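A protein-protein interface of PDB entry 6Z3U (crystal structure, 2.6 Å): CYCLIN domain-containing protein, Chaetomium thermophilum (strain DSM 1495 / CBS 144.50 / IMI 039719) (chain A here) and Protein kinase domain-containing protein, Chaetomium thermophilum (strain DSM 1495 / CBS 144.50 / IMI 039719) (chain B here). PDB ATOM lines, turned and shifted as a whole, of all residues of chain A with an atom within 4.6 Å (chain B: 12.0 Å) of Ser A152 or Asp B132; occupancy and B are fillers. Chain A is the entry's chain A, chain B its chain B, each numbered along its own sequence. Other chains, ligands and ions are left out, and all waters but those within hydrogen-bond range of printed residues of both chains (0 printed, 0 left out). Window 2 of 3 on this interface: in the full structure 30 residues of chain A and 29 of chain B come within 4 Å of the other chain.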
ATOM      1  N   PHE A 141     -29.022  20.396  -3.724  1.00  0.00           N
ATOM      2  CA  PHE A 141     -28.402  20.279  -5.039  1.00  0.00           C
ATOM      3  C   PHE A 141     -29.033  21.247  -6.030  1.00  0.00           C
ATOM      4  O   PHE A 141     -28.327  21.929  -6.782  1.00  0.00           O
ATOM      5  CB  PHE A 141     -28.517  18.842  -5.545  1.00  0.00           C
ATOM      6  CG  PHE A 141     -27.851  18.614  -6.871  1.00  0.00           C
ATOM      7  CD1 PHE A 141     -26.472  18.641  -6.980  1.00  0.00           C
ATOM      8  CD2 PHE A 141     -28.605  18.363  -8.004  1.00  0.00           C
ATOM      9  CE1 PHE A 141     -25.857  18.427  -8.196  1.00  0.00           C
ATOM     10  CE2 PHE A 141     -27.995  18.146  -9.221  1.00  0.00           C
ATOM     11  CZ  PHE A 141     -26.619  18.179  -9.318  1.00  0.00           C
ATOM     12  N   LYS A 145     -27.724  25.043  -8.191  1.00  0.00           N
ATOM     13  CA  LYS A 145     -27.964  25.415  -9.580  1.00  0.00           C
ATOM     14  C   LYS A 145     -28.723  26.732  -9.667  1.00  0.00           C
ATOM     15  O   LYS A 145     -28.370  27.617 -10.455  1.00  0.00           O
ATOM     16  CB  LYS A 145     -28.735  24.297 -10.282  1.00  0.00           C
ATOM     17  CG  LYS A 145     -27.975  22.981 -10.375  1.00  0.00           C
ATOM     18  CD  LYS A 145     -28.748  21.950 -11.186  1.00  0.00           C
ATOM     19  CE  LYS A 145     -27.865  20.778 -11.572  1.00  0.00           C
ATOM     20  NZ  LYS A 145     -28.611  19.735 -12.332  1.00  0.00           N
ATOM     21  N   PHE A 150     -23.180  24.931 -10.363  1.00  0.00           N
ATOM     22  CA  PHE A 150     -23.562  23.703 -11.057  1.00  0.00           C
ATOM     23  C   PHE A 150     -22.474  22.665 -10.812  1.00  0.00           C
ATOM     24  O   PHE A 150     -21.601  22.448 -11.665  1.00  0.00           O
ATOM     25  CB  PHE A 150     -23.775  23.954 -12.548  1.00  0.00           C
ATOM     26  CG  PHE A 150     -24.884  24.924 -12.841  1.00  0.00           C
ATOM     27  CD1 PHE A 150     -26.189  24.480 -12.980  1.00  0.00           C
ATOM     28  CD2 PHE A 150     -24.627  26.279 -12.963  1.00  0.00           C
ATOM     29  CE1 PHE A 150     -27.214  25.367 -13.242  1.00  0.00           C
ATOM     30  CE2 PHE A 150     -25.652  27.170 -13.226  1.00  0.00           C
ATOM     31  CZ  PHE A 150     -26.946  26.710 -13.365  1.00  0.00           C
ATOM     32  N   PRO A 151     -22.489  22.012  -9.654  1.00  0.00           N
ATOM     33  CA  PRO A 151     -21.464  21.011  -9.349  1.00  0.00           C
ATOM     34  C   PRO A 151     -21.769  19.681 -10.023  1.00  0.00           C
ATOM     35  O   PRO A 151     -22.865  19.438 -10.526  1.00  0.00           O
ATOM     36  CB  PRO A 151     -21.543  20.890  -7.825  1.00  0.00           C
ATOM     37  CG  PRO A 151     -22.977  21.175  -7.518  1.00  0.00           C
ATOM     38  CD  PRO A 151     -23.429  22.199  -8.532  1.00  0.00           C
ATOM     39  N   SER A 152     -20.764  18.811 -10.017  1.00  0.00           N
ATOM     40  CA  SER A 152     -20.933  17.458 -10.525  1.00  0.00           C
ATOM     41  C   SER A 152     -21.666  16.627  -9.481  1.00  0.00           C
ATOM     42  O   SER A 152     -21.308  16.645  -8.299  1.00  0.00           O
ATOM     43  CB  SER A 152     -19.580  16.832 -10.862  1.00  0.00           C
ATOM     44  OG  SER A 152     -19.742  15.566 -11.482  1.00  0.00           O
ATOM     45  N   ILE A 153     -22.690  15.893  -9.919  1.00  0.00           N
ATOM     46  CA  ILE A 153     -23.501  15.133  -8.973  1.00  0.00           C
ATOM     47  C   ILE A 153     -22.640  14.146  -8.200  1.00  0.00           C
ATOM     48  O   ILE A 153     -22.907  13.864  -7.025  1.00  0.00           O
ATOM     49  CB  ILE A 153     -24.656  14.427  -9.710  1.00  0.00           C
ATOM     50  CG1 ILE A 153     -25.628  13.791  -8.713  1.00  0.00           C
ATOM     51  CG2 ILE A 153     -24.118  13.371 -10.664  1.00  0.00           C
ATOM     52  CD1 ILE A 153     -26.281  14.778  -7.766  1.00  0.00           C
ATOM     53  N   SER A 154     -21.588  13.616  -8.828  1.00  0.00           N
ATOM     54  CA  SER A 154     -20.699  12.699  -8.120  1.00  0.00           C
ATOM     55  C   SER A 154     -19.980  13.406  -6.979  1.00  0.00           C
ATOM     56  O   SER A 154     -19.846  12.851  -5.882  1.00  0.00           O
ATOM     57  CB  SER A 154     -19.692  12.087  -9.093  1.00  0.00           C
ATOM     58  OG  SER A 154     -18.859  13.083  -9.658  1.00  0.00           O
ATOM     59  N   ASP A 155     -19.511  14.634  -7.215  1.00  0.00           N
ATOM     60  CA  ASP A 155     -18.851  15.386  -6.152  1.00  0.00           C
ATOM     61  C   ASP A 155     -19.845  15.797  -5.074  1.00  0.00           C
ATOM     62  O   ASP A 155     -19.516  15.788  -3.882  1.00  0.00           O
ATOM     63  CB  ASP A 155     -18.154  16.619  -6.727  1.00  0.00           C
ATOM     64  CG  ASP A 155     -17.003  16.266  -7.653  1.00  0.00           C
ATOM     65  OD1 ASP A 155     -16.415  15.176  -7.487  1.00  0.00           O
ATOM     66  OD2 ASP A 155     -16.682  17.083  -8.541  1.00  0.00           O
ATOM     67  N   PHE A 156     -21.063  16.173  -5.475  1.00  0.00           N
ATOM     68  CA  PHE A 156     -22.087  16.528  -4.498  1.00  0.00           C
ATOM     69  C   PHE A 156     -22.408  15.345  -3.592  1.00  0.00           C
ATOM     70  O   PHE A 156     -22.560  15.507  -2.376  1.00  0.00           O
ATOM     71  CB  PHE A 156     -23.347  17.018  -5.213  1.00  0.00           C
ATOM     72  CG  PHE A 156     -24.426  17.494  -4.281  1.00  0.00           C
ATOM     73  CD1 PHE A 156     -24.535  18.836  -3.960  1.00  0.00           C
ATOM     74  CD2 PHE A 156     -25.327  16.602  -3.726  1.00  0.00           C
ATOM     75  CE1 PHE A 156     -25.524  19.280  -3.102  1.00  0.00           C
ATOM     76  CE2 PHE A 156     -26.316  17.039  -2.866  1.00  0.00           C
ATOM     77  CZ  PHE A 156     -26.414  18.381  -2.555  1.00  0.00           C
ATOM     78  N   LEU A 169     -30.611  12.597  -8.139  1.00  0.00           N
ATOM     79  CA  LEU A 169     -31.134  13.126  -9.394  1.00  0.00           C
ATOM     80  C   LEU A 169     -32.600  12.767  -9.595  1.00  0.00           C
ATOM     81  O   LEU A 169     -33.342  13.522 -10.232  1.00  0.00           O
ATOM     82  CB  LEU A 169     -30.307  12.601 -10.567  1.00  0.00           C
ATOM     83  CG  LEU A 169     -28.824  12.966 -10.582  1.00  0.00           C
ATOM     84  CD1 LEU A 169     -28.140  12.310 -11.769  1.00  0.00           C
ATOM     85  CD2 LEU A 169     -28.635  14.469 -10.620  1.00  0.00           C
ATOM     86  N   LYS B 125     -35.578  18.790 -23.875  1.00  0.00           N
ATOM     87  CA  LYS B 125     -35.386  17.378 -23.560  1.00  0.00           C
ATOM     88  C   LYS B 125     -34.537  17.330 -22.298  1.00  0.00           C
ATOM     89  O   LYS B 125     -33.309  17.424 -22.354  1.00  0.00           O
ATOM     90  CB  LYS B 125     -34.733  16.646 -24.722  1.00  0.00           C
ATOM     91  CG  LYS B 125     -35.491  16.786 -26.035  1.00  0.00           C
ATOM     92  CD  LYS B 125     -34.922  15.877 -27.116  1.00  0.00           C
ATOM     93  CE  LYS B 125     -35.690  16.021 -28.424  1.00  0.00           C
ATOM     94  NZ  LYS B 125     -35.308  14.984 -29.424  1.00  0.00           N
ATOM     95  N   VAL B 126     -35.208  17.191 -21.150  1.00  0.00           N
ATOM     96  CA  VAL B 126     -34.528  17.197 -19.856  1.00  0.00           C
ATOM     97  C   VAL B 126     -33.356  16.230 -19.849  1.00  0.00           C
ATOM     98  O   VAL B 126     -32.379  16.433 -19.117  1.00  0.00           O
ATOM     99  CB  VAL B 126     -35.544  16.885 -18.730  1.00  0.00           C
ATOM    100  CG1 VAL B 126     -34.985  15.871 -17.729  1.00  0.00           C
ATOM    101  CG2 VAL B 126     -35.947  18.173 -18.017  1.00  0.00           C
ATOM    102  N   GLN B 127     -33.419  15.178 -20.663  1.00  0.00           N
ATOM    103  CA  GLN B 127     -32.323  14.223 -20.799  1.00  0.00           C
ATOM    104  C   GLN B 127     -31.687  14.486 -22.165  1.00  0.00           C
ATOM    105  O   GLN B 127     -32.193  14.031 -23.194  1.00  0.00           O
ATOM    106  CB  GLN B 127     -32.809  12.781 -20.662  1.00  0.00           C
ATOM    107  CG  GLN B 127     -34.026  12.391 -21.505  1.00  0.00           C
ATOM    108  CD  GLN B 127     -35.352  12.750 -20.859  1.00  0.00           C
ATOM    109  OE1 GLN B 127     -35.491  12.721 -19.635  1.00  0.00           O
ATOM    110  NE2 GLN B 127     -36.348  13.056 -21.685  1.00  0.00           N
ATOM    111  N   ALA B 128     -30.579  15.231 -22.167  1.00  0.00           N
ATOM    112  CA  ALA B 128     -29.865  15.588 -23.392  1.00  0.00           C
ATOM    113  C   ALA B 128     -28.371  15.297 -23.220  1.00  0.00           C
ATOM    114  O   ALA B 128     -27.520  16.185 -23.257  1.00  0.00           O
ATOM    115  CB  ALA B 128     -30.104  17.051 -23.761  1.00  0.00           C
ATOM    116  N   GLN B 129     -28.066  14.015 -23.020  1.00  0.00           N
ATOM    117  CA  GLN B 129     -26.706  13.488 -22.911  1.00  0.00           C
ATOM    118  C   GLN B 129     -25.942  14.090 -21.727  1.00  0.00           C
ATOM    119  O   GLN B 129     -24.708  14.105 -21.720  1.00  0.00           O
ATOM    120  CB  GLN B 129     -25.928  13.704 -24.217  1.00  0.00           C
ATOM    121  CG  GLN B 129     -24.949  12.578 -24.537  1.00  0.00           C
ATOM    122  CD  GLN B 129     -23.684  12.617 -23.711  1.00  0.00           C
ATOM    123  OE1 GLN B 129     -22.983  13.628 -23.663  1.00  0.00           O
ATOM    124  NE2 GLN B 129     -23.404  11.517 -23.020  1.00  0.00           N
ATOM    125  N   TYR B 130     -26.652  14.608 -20.729  1.00  0.00           N
ATOM    126  CA  TYR B 130     -26.059  15.237 -19.551  1.00  0.00           C
ATOM    127  C   TYR B 130     -26.215  14.325 -18.342  1.00  0.00           C
ATOM    128  O   TYR B 130     -27.340  13.992 -17.951  1.00  0.00           O
ATOM    129  CB  TYR B 130     -26.691  16.607 -19.297  1.00  0.00           C
ATOM    130  CG  TYR B 130     -25.868  17.521 -18.413  1.00  0.00           C
ATOM    131  CD1 TYR B 130     -24.485  17.590 -18.531  1.00  0.00           C
ATOM    132  CD2 TYR B 130     -26.486  18.352 -17.486  1.00  0.00           C
ATOM    133  CE1 TYR B 130     -23.740  18.428 -17.723  1.00  0.00           C
ATOM    134  CE2 TYR B 130     -25.750  19.201 -16.683  1.00  0.00           C
ATOM    135  CZ  TYR B 130     -24.379  19.238 -16.807  1.00  0.00           C
ATOM    136  OH  TYR B 130     -23.646  20.083 -16.004  1.00  0.00           O
ATOM    137  N   LYS B 131     -25.090  13.927 -17.749  1.00  0.00           N
ATOM    138  CA  LYS B 131     -25.102  12.987 -16.639  1.00  0.00           C
ATOM    139  C   LYS B 131     -25.219  13.662 -15.277  1.00  0.00           C
ATOM    140  O   LYS B 131     -25.235  12.962 -14.259  1.00  0.00           O
ATOM    141  CB  LYS B 131     -23.825  12.132 -16.658  1.00  0.00           C
ATOM    142  CG  LYS B 131     -23.444  11.565 -18.025  1.00  0.00           C
ATOM    143  CD  LYS B 131     -22.651  10.268 -17.894  1.00  0.00           C
ATOM    144  CE  LYS B 131     -23.600   9.074 -17.809  1.00  0.00           C
ATOM    145  NZ  LYS B 131     -22.927   7.793 -17.456  1.00  0.00           N
ATOM    146  N   ASP B 132     -25.305  14.992 -15.225  1.00  0.00           N
ATOM    147  CA  ASP B 132     -25.391  15.724 -13.966  1.00  0.00           C
ATOM    148  C   ASP B 132     -26.774  16.331 -13.730  1.00  0.00           C
ATOM    149  O   ASP B 132     -26.900  17.353 -13.053  1.00  0.00           O
ATOM    150  CB  ASP B 132     -24.325  16.818 -13.922  1.00  0.00           C
ATOM    151  CG  ASP B 132     -22.928  16.275 -14.139  1.00  0.00           C
ATOM    152  OD1 ASP B 132     -22.159  16.196 -13.159  1.00  0.00           O
ATOM    153  OD2 ASP B 132     -22.607  15.901 -15.287  1.00  0.00           O
ATOM    154  N   GLY B 133     -27.820  15.712 -14.274  1.00  0.00           N
ATOM    155  CA  GLY B 133     -29.163  16.208 -14.039  1.00  0.00           C
ATOM    156  C   GLY B 133     -29.551  17.317 -15.005  1.00  0.00           C
ATOM    157  O   GLY B 133     -29.120  17.355 -16.158  1.00  0.00           O
ATOM    158  N   MET B 134     -30.390  18.231 -14.514  1.00  0.00           N
ATOM    159  CA  MET B 134     -30.889  19.319 -15.345  1.00  0.00           C
ATOM    160  C   MET B 134     -29.741  20.196 -15.832  1.00  0.00           C
ATOM    161  O   MET B 134     -28.868  20.588 -15.052  1.00  0.00           O
ATOM    162  CB  MET B 134     -31.901  20.158 -14.561  1.00  0.00           C
ATOM    163  CG  MET B 134     -32.648  21.172 -15.420  1.00  0.00           C
ATOM    164  SD  MET B 134     -34.042  21.982 -14.605  1.00  0.00           S
ATOM    165  CE  MET B 134     -34.883  20.599 -13.832  1.00  0.00           C
ATOM    166  N   ALA B 135     -29.755  20.515 -17.124  1.00  0.00           N
ATOM    167  CA  ALA B 135     -28.664  21.267 -17.720  1.00  0.00           C
ATOM    168  C   ALA B 135     -28.693  22.726 -17.261  1.00  0.00           C
ATOM    169  O   ALA B 135     -29.764  23.293 -17.026  1.00  0.00           O
ATOM    170  CB  ALA B 135     -28.745  21.205 -19.243  1.00  0.00           C
ATOM    171  N   PRO B 136     -27.522  23.362 -17.138  1.00  0.00           N
ATOM    172  CA  PRO B 136     -27.505  24.754 -16.657  1.00  0.00           C
ATOM    173  C   PRO B 136     -28.232  25.722 -17.573  1.00  0.00           C
ATOM    174  O   PRO B 136     -28.866  26.667 -17.087  1.00  0.00           O
ATOM    175  CB  PRO B 136     -26.004  25.078 -16.560  1.00  0.00           C
ATOM    176  CG  PRO B 136     -25.319  24.054 -17.402  1.00  0.00           C
ATOM    177  CD  PRO B 136     -26.165  22.827 -17.350  1.00  0.00           C
ATOM    178  N   ASP B 137     -28.164  25.520 -18.890  1.00  0.00           N
ATOM    179  CA  ASP B 137     -28.887  26.404 -19.796  1.00  0.00           C
ATOM    180  C   ASP B 137     -30.388  26.341 -19.550  1.00  0.00           C
ATOM    181  O   ASP B 137     -31.093  27.336 -19.750  1.00  0.00           O
ATOM    182  CB  ASP B 137     -28.566  26.045 -21.247  1.00  0.00           C
ATOM    183  CG  ASP B 137     -28.801  24.579 -21.552  1.00  0.00           C
ATOM    184  OD1 ASP B 137     -28.986  23.798 -20.598  1.00  0.00           O
ATOM    185  OD2 ASP B 137     -28.797  24.206 -22.743  1.00  0.00           O
ATOM    186  N   ALA B 138     -30.895  25.186 -19.116  1.00  0.00           N
ATOM    187  CA  ALA B 138     -32.315  25.072 -18.801  1.00  0.00           C
ATOM    188  C   ALA B 138     -32.649  25.803 -17.508  1.00  0.00           C
ATOM    189  O   ALA B 138     -33.627  26.557 -17.442  1.00  0.00           O
ATOM    190  CB  ALA B 138     -32.711  23.599 -18.703  1.00  0.00           C
ATOM    191  N   VAL B 139     -31.840  25.596 -16.465  1.00  0.00           N
ATOM    192  CA  VAL B 139     -32.090  26.256 -15.187  1.00  0.00           C
ATOM    193  C   VAL B 139     -32.005  27.769 -15.339  1.00  0.00           C
ATOM    194  O   VAL B 139     -32.833  28.511 -14.793  1.00  0.00           O
ATOM    195  CB  VAL B 139     -31.098  25.741 -14.127  1.00  0.00           C
ATOM    196  CG1 VAL B 139     -31.212  26.556 -12.860  1.00  0.00           C
ATOM    197  CG2 VAL B 139     -31.346  24.275 -13.843  1.00  0.00           C
ATOM    198  N   ARG B 140     -31.005  28.251 -16.078  1.00  0.00           N
ATOM    199  CA  ARG B 140     -30.813  29.691 -16.221  1.00  0.00           C
ATOM    200  C   ARG B 140     -31.974  30.329 -16.974  1.00  0.00           C
ATOM    201  O   ARG B 140     -32.503  31.365 -16.555  1.00  0.00           O
ATOM    202  CB  ARG B 140     -29.487  29.974 -16.930  1.00  0.00           C
ATOM    203  CG  ARG B 140     -28.262  29.752 -16.055  1.00  0.00           C
ATOM    204  CD  ARG B 140     -26.984  29.640 -16.867  1.00  0.00           C
ATOM    205  NE  ARG B 140     -25.808  29.576 -16.002  1.00  0.00           N
ATOM    206  CZ  ARG B 140     -24.652  29.011 -16.339  1.00  0.00           C
ATOM    207  NH1 ARG B 140     -24.504  28.435 -17.526  1.00  0.00           N
ATOM    208  NH2 ARG B 140     -23.642  29.014 -15.479  1.00  0.00           N
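The side-chain carboxylate (OD1) of Asp B132 is in hydrogen-bond range of the side-chain hydroxyl (OG) of Ser A152. NZ of Lys A145 is in hydrogen-bond range of O of Asp B132 (3.0 Å). The backbone NH of Ile A153 is in hydrogen-bond range of the side-chain carboxylate of Asp B132 (3.3 Å). The side-chain amino group (NZ) of Lys A145 sits at hydrogen-bond distance from the backbone carbonyl oxygen (O) of Met B134 (2.9 Å).
OG of Ser A154 sits at hydrogen-bond distance from OG of Ser A152 (3.2 Å).
Phe A141 touches Asp B132. Lys A145 touches Gly B133. O of Lys A145 touches CG1 of Val B139, at 3.9 Å. Phe A150 touches Pro B136. Phe A150 touches Arg B140. Lys B131 touches Ile A153 (O to CG2, 3.8 Å). O of Lys B131 touches CD1 of Leu A169 (3.9 Å). CA of Gly B133 touches CD2 of Leu A169, 3.9 Å away.
Ser A152 touches just one residue of chain B: Asp B132. Of chain A, only Phe A141 (3.8 Å), Lys A145 (3.0 Å), Ser A152 (3.0 Å) and Ile A153 (3.3 Å) come within 4 Å of Asp B132. No residue of chain B comes within 4 Å of Pro A151. No residue of chain B comes within 4 Å of Phe A156. Of the printed residues of chain B, Leu A169 touches Lys B131 (3.9 Å) and Gly B133 (3.9 Å). Of the printed residues of chain B, Lys A145 touches Asp B132, Gly B133, Met B134 and Val B139. Of the printed residues of chain A, Met B134 touches Lys A145. Printed residues of chain A within 4 Å of Lys B131: Ile A153 (3.8 Å) and Leu A169 (3.9 Å). Printed residues of chain B within 4 Å of Phe A141: Asp B132. Ala B128 touches none of the printed residues of chain A. Val B126 touches none of the printed residues of chain A. The nearest printed residue of chain B that does not touch Ser A152 is Tyr B130 (6.7 Å). The nearest residue of chain A that does not touch Asp B132 is Leu A169 (4.1 Å).
Of the 10 printed residues of chain A, 6 touch a printed residue of chain B. Printed residues of chain A that touch a printed residue of chain B: Phe A141, Lys A145, Phe A150, Ser A152, Ile A153 and Leu A169. Hydrophobic or aromatic side chains of chain A that line the printed part of chain B: Phe A141, Phe A150, Ile A153 and Leu A169. Printed residues of chain B that touch a printed residue of chain A: Lys B131, Asp B132, Gly B133, Met B134, Pro B136, Val B139 and Arg B140. Among the printed residues, no Asp or Glu carboxylate lies within 4 Å of a Lys or Arg side-chain nitrogen of the other chain.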
